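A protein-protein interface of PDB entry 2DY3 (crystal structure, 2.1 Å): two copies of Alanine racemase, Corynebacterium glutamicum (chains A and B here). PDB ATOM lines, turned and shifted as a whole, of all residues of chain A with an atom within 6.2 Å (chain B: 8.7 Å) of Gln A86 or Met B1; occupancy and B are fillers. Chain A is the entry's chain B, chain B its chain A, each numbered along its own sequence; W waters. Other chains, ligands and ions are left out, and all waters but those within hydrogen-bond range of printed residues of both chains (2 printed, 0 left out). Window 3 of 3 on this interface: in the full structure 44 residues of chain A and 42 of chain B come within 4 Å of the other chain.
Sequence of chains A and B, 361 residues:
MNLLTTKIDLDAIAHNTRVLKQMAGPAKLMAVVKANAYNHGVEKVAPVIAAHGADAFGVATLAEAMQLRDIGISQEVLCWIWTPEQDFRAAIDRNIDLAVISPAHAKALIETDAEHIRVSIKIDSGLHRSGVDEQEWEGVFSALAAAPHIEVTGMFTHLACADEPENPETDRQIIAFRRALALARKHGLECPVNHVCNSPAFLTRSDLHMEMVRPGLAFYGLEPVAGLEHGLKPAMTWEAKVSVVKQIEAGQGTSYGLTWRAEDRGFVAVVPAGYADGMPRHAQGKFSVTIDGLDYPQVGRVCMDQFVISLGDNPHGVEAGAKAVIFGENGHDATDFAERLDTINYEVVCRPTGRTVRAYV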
ATOM      1  N   LEU A  62      -3.885  16.637   1.676  1.00  0.00           N
ATOM      2  CA  LEU A  62      -4.449  16.355   0.368  1.00  0.00           C
ATOM      3  C   LEU A  62      -4.033  14.951  -0.031  1.00  0.00           C
ATOM      4  O   LEU A  62      -4.844  14.160  -0.511  1.00  0.00           O
ATOM      5  CB  LEU A  62      -3.887  17.353  -0.644  1.00  0.00           C
ATOM      6  CG  LEU A  62      -4.703  18.522  -1.200  1.00  0.00           C
ATOM      7  CD1 LEU A  62      -5.844  18.915  -0.273  1.00  0.00           C
ATOM      8  CD2 LEU A  62      -3.747  19.683  -1.454  1.00  0.00           C
ATOM      9  N   ILE A  81      -5.561  20.290   6.089  1.00  0.00           N
ATOM     10  CA  ILE A  81      -4.245  20.924   6.041  1.00  0.00           C
ATOM     11  C   ILE A  81      -3.715  20.926   4.613  1.00  0.00           C
ATOM     12  O   ILE A  81      -3.178  19.930   4.129  1.00  0.00           O
ATOM     13  CB  ILE A  81      -3.212  20.218   6.962  1.00  0.00           C
ATOM     14  CG1 ILE A  81      -3.652  20.325   8.423  1.00  0.00           C
ATOM     15  CG2 ILE A  81      -1.859  20.884   6.823  1.00  0.00           C
ATOM     16  CD1 ILE A  81      -2.674  19.699   9.410  1.00  0.00           C
ATOM     17  N   TRP A  82      -3.890  22.059   3.944  1.00  0.00           N
ATOM     18  CA  TRP A  82      -3.446  22.245   2.567  1.00  0.00           C
ATOM     19  C   TRP A  82      -3.290  23.740   2.346  1.00  0.00           C
ATOM     20  O   TRP A  82      -3.719  24.533   3.178  1.00  0.00           O
ATOM     21  CB  TRP A  82      -4.494  21.712   1.582  1.00  0.00           C
ATOM     22  CG  TRP A  82      -5.855  22.359   1.723  1.00  0.00           C
ATOM     23  CD1 TRP A  82      -6.798  22.082   2.671  1.00  0.00           C
ATOM     24  CD2 TRP A  82      -6.424  23.378   0.882  1.00  0.00           C
ATOM     25  NE1 TRP A  82      -7.918  22.857   2.471  1.00  0.00           N
ATOM     26  CE2 TRP A  82      -7.714  23.661   1.380  1.00  0.00           C
ATOM     27  CE3 TRP A  82      -5.969  24.076  -0.244  1.00  0.00           C
ATOM     28  CZ2 TRP A  82      -8.557  24.613   0.791  1.00  0.00           C
ATOM     29  CZ3 TRP A  82      -6.802  25.021  -0.826  1.00  0.00           C
ATOM     30  CH2 TRP A  82      -8.083  25.281  -0.307  1.00  0.00           C
ATOM     31  N   THR A  83      -2.662  24.119   1.238  1.00  0.00           N
ATOM     32  CA  THR A  83      -2.486  25.525   0.903  1.00  0.00           C
ATOM     33  C   THR A  83      -2.876  25.692  -0.551  1.00  0.00           C
ATOM     34  O   THR A  83      -2.799  24.751  -1.334  1.00  0.00           O
ATOM     35  CB  THR A  83      -1.025  26.002   1.080  1.00  0.00           C
ATOM     36  OG1 THR A  83      -0.175  25.276   0.181  1.00  0.00           O
ATOM     37  CG2 THR A  83      -0.563  25.794   2.527  1.00  0.00           C
ATOM     38  N   PRO A  84      -3.299  26.901  -0.932  1.00  0.00           N
ATOM     39  CA  PRO A  84      -3.712  27.209  -2.305  1.00  0.00           C
ATOM     40  C   PRO A  84      -2.595  27.001  -3.313  1.00  0.00           C
ATOM     41  O   PRO A  84      -2.838  26.951  -4.520  1.00  0.00           O
ATOM     42  CB  PRO A  84      -4.135  28.673  -2.216  1.00  0.00           C
ATOM     43  CG  PRO A  84      -4.621  28.796  -0.795  1.00  0.00           C
ATOM     44  CD  PRO A  84      -3.554  28.046  -0.039  1.00  0.00           C
ATOM     45  N   GLU A  85      -1.372  26.881  -2.814  1.00  0.00           N
ATOM     46  CA  GLU A  85      -0.214  26.691  -3.674  1.00  0.00           C
ATOM     47  C   GLU A  85      -0.104  25.242  -4.145  1.00  0.00           C
ATOM     48  O   GLU A  85       0.607  24.946  -5.106  1.00  0.00           O
ATOM     49  CB  GLU A  85       1.065  27.102  -2.935  1.00  0.00           C
ATOM     50  CG  GLU A  85       1.123  28.581  -2.511  1.00  0.00           C
ATOM     51  CD  GLU A  85       0.164  28.935  -1.370  1.00  0.00           C
ATOM     52  OE1 GLU A  85      -1.065  28.881  -1.574  1.00  0.00           O
ATOM     53  OE2 GLU A  85       0.641  29.271  -0.261  1.00  0.00           O
ATOM     54  N   GLN A  86      -0.801  24.337  -3.465  1.00  0.00           N
ATOM     55  CA  GLN A  86      -0.771  22.931  -3.845  1.00  0.00           C
ATOM     56  C   GLN A  86      -1.854  22.663  -4.876  1.00  0.00           C
ATOM     57  O   GLN A  86      -2.692  23.522  -5.142  1.00  0.00           O
ATOM     58  CB  GLN A  86      -1.026  22.032  -2.638  1.00  0.00           C
ATOM     59  CG  GLN A  86      -0.169  22.328  -1.428  1.00  0.00           C
ATOM     60  CD  GLN A  86      -0.351  21.282  -0.356  1.00  0.00           C
ATOM     61  OE1 GLN A  86       0.329  20.248  -0.351  1.00  0.00           O
ATOM     62  NE2 GLN A  86      -1.288  21.529   0.547  1.00  0.00           N
ATOM     63  N   ASP A  87      -1.846  21.463  -5.441  1.00  0.00           N
ATOM     64  CA  ASP A  87      -2.850  21.082  -6.429  1.00  0.00           C
ATOM     65  C   ASP A  87      -4.111  20.602  -5.700  1.00  0.00           C
ATOM     66  O   ASP A  87      -4.439  19.412  -5.726  1.00  0.00           O
ATOM     67  CB  ASP A  87      -2.306  19.962  -7.322  1.00  0.00           C
ATOM     68  CG  ASP A  87      -3.238  19.623  -8.468  1.00  0.00           C
ATOM     69  OD1 ASP A  87      -2.894  18.735  -9.271  1.00  0.00           O
ATOM     70  OD2 ASP A  87      -4.310  20.247  -8.571  1.00  0.00           O
ATOM     71  N   PHE A  88      -4.817  21.521  -5.047  1.00  0.00           N
ATOM     72  CA  PHE A  88      -6.023  21.152  -4.322  1.00  0.00           C
ATOM     73  C   PHE A  88      -7.137  20.779  -5.293  1.00  0.00           C
ATOM     74  O   PHE A  88      -8.050  20.036  -4.941  1.00  0.00           O
ATOM     75  CB  PHE A  88      -6.465  22.298  -3.397  1.00  0.00           C
ATOM     76  CG  PHE A  88      -6.819  23.565  -4.117  1.00  0.00           C
ATOM     77  CD1 PHE A  88      -8.103  23.774  -4.590  1.00  0.00           C
ATOM     78  CD2 PHE A  88      -5.871  24.556  -4.310  1.00  0.00           C
ATOM     79  CE1 PHE A  88      -8.441  24.950  -5.240  1.00  0.00           C
ATOM     80  CE2 PHE A  88      -6.201  25.736  -4.963  1.00  0.00           C
ATOM     81  CZ  PHE A  88      -7.490  25.928  -5.426  1.00  0.00           C
ATOM     82  N   ARG A  89      -7.046  21.288  -6.519  1.00  0.00           N
ATOM     83  CA  ARG A  89      -8.028  20.995  -7.555  1.00  0.00           C
ATOM     84  C   ARG A  89      -8.057  19.494  -7.794  1.00  0.00           C
ATOM     85  O   ARG A  89      -9.107  18.922  -8.085  1.00  0.00           O
ATOM     86  CB  ARG A  89      -7.671  21.723  -8.864  1.00  0.00           C
ATOM     87  CG  ARG A  89      -8.537  21.325 -10.066  1.00  0.00           C
ATOM     88  CD  ARG A  89     -10.021  21.512  -9.776  1.00  0.00           C
ATOM     89  NE  ARG A  89     -10.862  20.964 -10.837  1.00  0.00           N
ATOM     90  CZ  ARG A  89     -11.132  21.583 -11.985  1.00  0.00           C
ATOM     91  NH1 ARG A  89     -10.635  22.789 -12.231  1.00  0.00           N
ATOM     92  NH2 ARG A  89     -11.900  20.992 -12.894  1.00  0.00           N
ATOM     93  N   MET B   1       3.065  20.177  -5.051  1.00  0.00           N
ATOM     94  CA  MET B   1       4.010  20.684  -4.015  1.00  0.00           C
ATOM     95  C   MET B   1       3.737  20.072  -2.644  1.00  0.00           C
ATOM     96  O   MET B   1       2.588  19.842  -2.272  1.00  0.00           O
ATOM     97  CB  MET B   1       3.923  22.206  -3.918  1.00  0.00           C
ATOM     98  CG  MET B   1       4.767  22.778  -2.799  1.00  0.00           C
ATOM     99  SD  MET B   1       3.787  23.589  -1.533  1.00  0.00           S
ATOM    100  CE  MET B   1       3.144  22.247  -0.644  1.00  0.00           C
ATOM    101  N   ASN B   2       4.806  19.826  -1.891  1.00  0.00           N
ATOM    102  CA  ASN B   2       4.697  19.235  -0.564  1.00  0.00           C
ATOM    103  C   ASN B   2       5.012  20.255   0.525  1.00  0.00           C
ATOM    104  O   ASN B   2       5.960  21.023   0.413  1.00  0.00           O
ATOM    105  CB  ASN B   2       5.639  18.041  -0.458  1.00  0.00           C
ATOM    106  CG  ASN B   2       5.400  17.027  -1.552  1.00  0.00           C
ATOM    107  OD1 ASN B   2       4.306  16.468  -1.671  1.00  0.00           O
ATOM    108  ND2 ASN B   2       6.419  16.790  -2.368  1.00  0.00           N
ATOM    109  N   LEU B   3       4.199  20.255   1.575  1.00  0.00           N
ATOM    110  CA  LEU B   3       4.354  21.196   2.682  1.00  0.00           C
ATOM    111  C   LEU B   3       5.487  20.824   3.628  1.00  0.00           C
ATOM    112  O   LEU B   3       5.931  21.647   4.424  1.00  0.00           O
ATOM    113  CB  LEU B   3       3.054  21.258   3.483  1.00  0.00           C
ATOM    114  CG  LEU B   3       1.760  21.594   2.735  1.00  0.00           C
ATOM    115  CD1 LEU B   3       0.570  21.332   3.651  1.00  0.00           C
ATOM    116  CD2 LEU B   3       1.786  23.038   2.271  1.00  0.00           C
ATOM    117  N   LEU B   4       5.942  19.578   3.538  1.00  0.00           N
ATOM    118  CA  LEU B   4       6.983  19.068   4.415  1.00  0.00           C
ATOM    119  C   LEU B   4       7.912  18.132   3.667  1.00  0.00           C
ATOM    120  O   LEU B   4       7.488  17.084   3.177  1.00  0.00           O
ATOM    121  CB  LEU B   4       6.340  18.318   5.581  1.00  0.00           C
ATOM    122  CG  LEU B   4       7.242  17.884   6.735  1.00  0.00           C
ATOM    123  CD1 LEU B   4       7.847  19.117   7.417  1.00  0.00           C
ATOM    124  CD2 LEU B   4       6.426  17.057   7.724  1.00  0.00           C
ATOM    125  N   THR B   5       9.189  18.491   3.608  1.00  0.00           N
ATOM    126  CA  THR B   5      10.141  17.671   2.881  1.00  0.00           C
ATOM    127  C   THR B   5      11.552  17.664   3.449  1.00  0.00           C
ATOM    128  O   THR B   5      11.908  18.485   4.289  1.00  0.00           O
ATOM    129  CB  THR B   5      10.273  18.167   1.428  1.00  0.00           C
ATOM    130  OG1 THR B   5      10.958  19.424   1.429  1.00  0.00           O
ATOM    131  CG2 THR B   5       8.906  18.378   0.796  1.00  0.00           C
ATOM    132  N   ALA B 240       9.685  23.094   6.023  1.00  0.00           N
ATOM    133  CA  ALA B 240       8.248  23.133   5.830  1.00  0.00           C
ATOM    134  C   ALA B 240       7.820  24.483   5.311  1.00  0.00           C
ATOM    135  O   ALA B 240       8.574  25.457   5.366  1.00  0.00           O
ATOM    136  CB  ALA B 240       7.528  22.853   7.144  1.00  0.00           C
ATOM    137  N   LYS B 241       6.597  24.527   4.803  1.00  0.00           N
ATOM    138  CA  LYS B 241       6.022  25.758   4.307  1.00  0.00           C
ATOM    139  C   LYS B 241       4.931  26.161   5.284  1.00  0.00           C
ATOM    140  O   LYS B 241       4.051  25.355   5.617  1.00  0.00           O
ATOM    141  CB  LYS B 241       5.431  25.547   2.912  1.00  0.00           C
ATOM    142  CG  LYS B 241       6.477  25.157   1.882  1.00  0.00           C
ATOM    143  CD  LYS B 241       6.048  25.518   0.481  1.00  0.00           C
ATOM    144  CE  LYS B 241       7.215  25.410  -0.485  1.00  0.00           C
ATOM    145  NZ  LYS B 241       6.841  25.889  -1.840  1.00  0.00           N
ATOM    146  N   VAL B 242       5.003  27.399   5.761  1.00  0.00           N
ATOM    147  CA  VAL B 242       4.008  27.904   6.694  1.00  0.00           C
ATOM    148  C   VAL B 242       2.649  27.734   6.035  1.00  0.00           C
ATOM    149  O   VAL B 242       2.455  28.118   4.881  1.00  0.00           O
ATOM    150  CB  VAL B 242       4.271  29.394   7.024  1.00  0.00           C
ATOM    151  CG1 VAL B 242       3.129  29.963   7.871  1.00  0.00           C
ATOM    152  CG2 VAL B 242       5.602  29.523   7.773  1.00  0.00           C
ATOM    153  N   SER B 243       1.715  27.133   6.758  1.00  0.00           N
ATOM    154  CA  SER B 243       0.377  26.896   6.222  1.00  0.00           C
ATOM    155  C   SER B 243      -0.576  28.054   6.485  1.00  0.00           C
ATOM    156  O   SER B 243      -1.492  28.292   5.704  1.00  0.00           O
ATOM    157  CB  SER B 243      -0.209  25.619   6.821  1.00  0.00           C
ATOM    158  OG  SER B 243      -0.418  25.778   8.210  1.00  0.00           O
ATOM    159  N   PRO B 272       3.217  23.002   9.347  1.00  0.00           N
ATOM    160  CA  PRO B 272       2.719  21.681   8.944  1.00  0.00           C
ATOM    161  C   PRO B 272       3.581  20.467   9.321  1.00  0.00           C
ATOM    162  O   PRO B 272       3.993  19.710   8.443  1.00  0.00           O
ATOM    163  CB  PRO B 272       2.584  21.808   7.421  1.00  0.00           C
ATOM    164  CG  PRO B 272       2.551  23.277   7.167  1.00  0.00           C
ATOM    165  CD  PRO B 272       3.514  23.827   8.166  1.00  0.00           C
ATOM    166  N   GLY B 321       3.031  30.071   3.288  1.00  0.00           N
ATOM    167  CA  GLY B 321       3.800  29.729   2.106  1.00  0.00           C
ATOM    168  C   GLY B 321       5.289  29.922   2.334  1.00  0.00           C
ATOM    169  O   GLY B 321       6.108  29.395   1.586  1.00  0.00           O
ATOM    170  N   ALA B 322       5.645  30.672   3.375  1.00  0.00           N
ATOM    171  CA  ALA B 322       7.050  30.924   3.685  1.00  0.00           C
ATOM    172  C   ALA B 322       7.798  29.626   3.992  1.00  0.00           C
ATOM    173  O   ALA B 322       7.229  28.680   4.543  1.00  0.00           O
ATOM    174  CB  ALA B 322       7.165  31.875   4.866  1.00  0.00           C
ATOM    175  N   VAL B 357       8.123  14.262   2.788  1.00  0.00           N
ATOM    176  CA  VAL B 357       8.438  13.698   1.479  1.00  0.00           C
ATOM    177  C   VAL B 357       9.903  13.967   1.157  1.00  0.00           C
ATOM    178  O   VAL B 357      10.364  15.110   1.231  1.00  0.00           O
ATOM    179  CB  VAL B 357       7.571  14.342   0.371  1.00  0.00           C
ATOM    180  CG1 VAL B 357       8.069  13.905  -0.998  1.00  0.00           C
ATOM    181  CG2 VAL B 357       6.118  13.955   0.558  1.00  0.00           C
HETATM  182  O   HOH W   1       0.269  19.658  -5.139  1.00  0.00           O
HETATM  183  O   HOH W   2       1.837  18.289   1.703  1.00  0.00           O
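Leu B3 touches Thr A83. Ser B243 touches Thr A83. Gly B321 touches Glu A85 (CA to OE2, 3.97 Å). CD1 of Leu B3 touches NE2 of Gln A86, 3.6 Å away.
Water W1 lies within hydrogen-bond range of N of Asp A87 (2.8 Å) and N of Met B1 (2.8 Å). Water W2 lies within hydrogen-bond range of N of Leu B3 (3.1 Å) and OE1 of Gln A86 (3.2 Å).
The side-chain amide oxygen (OE1) of Gln A86 sits close to the backbone carbonyl oxygen (O) of Met B1, 3.0 Å away.
Of chain B, only Met B1 (3.0 Å) and Leu B3 (3.6 Å) come within 4 Å of Gln A86. Met B1 touches just one residue of chain A: Gln A86 (3.0 Å). Printed residues of chain B within 4 Å of Glu A85: Gly B321. Of the printed residues of chain A, Gly B321 touches Glu A85 (3.97 Å). Lys B241 touches none of the printed residues of chain A. Trp A82 touches none of the printed residues of chain B. The nearest residue of chain B that does not touch Gln A86 is Asn B2 (4.5 Å). The nearest printed residue of chain A that does not touch Ser B243 is Ile A81 (5.0 Å).
Of the 10 printed residues of chain A, 3 touch a printed residue of chain B. Hydrophobic or aromatic side chains of chain B within 4 Å of the printed part of chain A: Met B1 and Leu B3. Among the printed residues, no Asp or Glu carboxylate lies within 4 Å of a Lys or Arg side-chain nitrogen of the other chain.
No position is printed for both chains.
The backbone NH of Gly B321 is in hydrogen-bond range of the backbone carbonyl oxygen of Val B242. NE2 of Gln A86 lies close to N of Thr A83, 3.0 Å away. O of Leu B3 lies within hydrogen-bond range of N of Lys B241 (3.0 Å).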
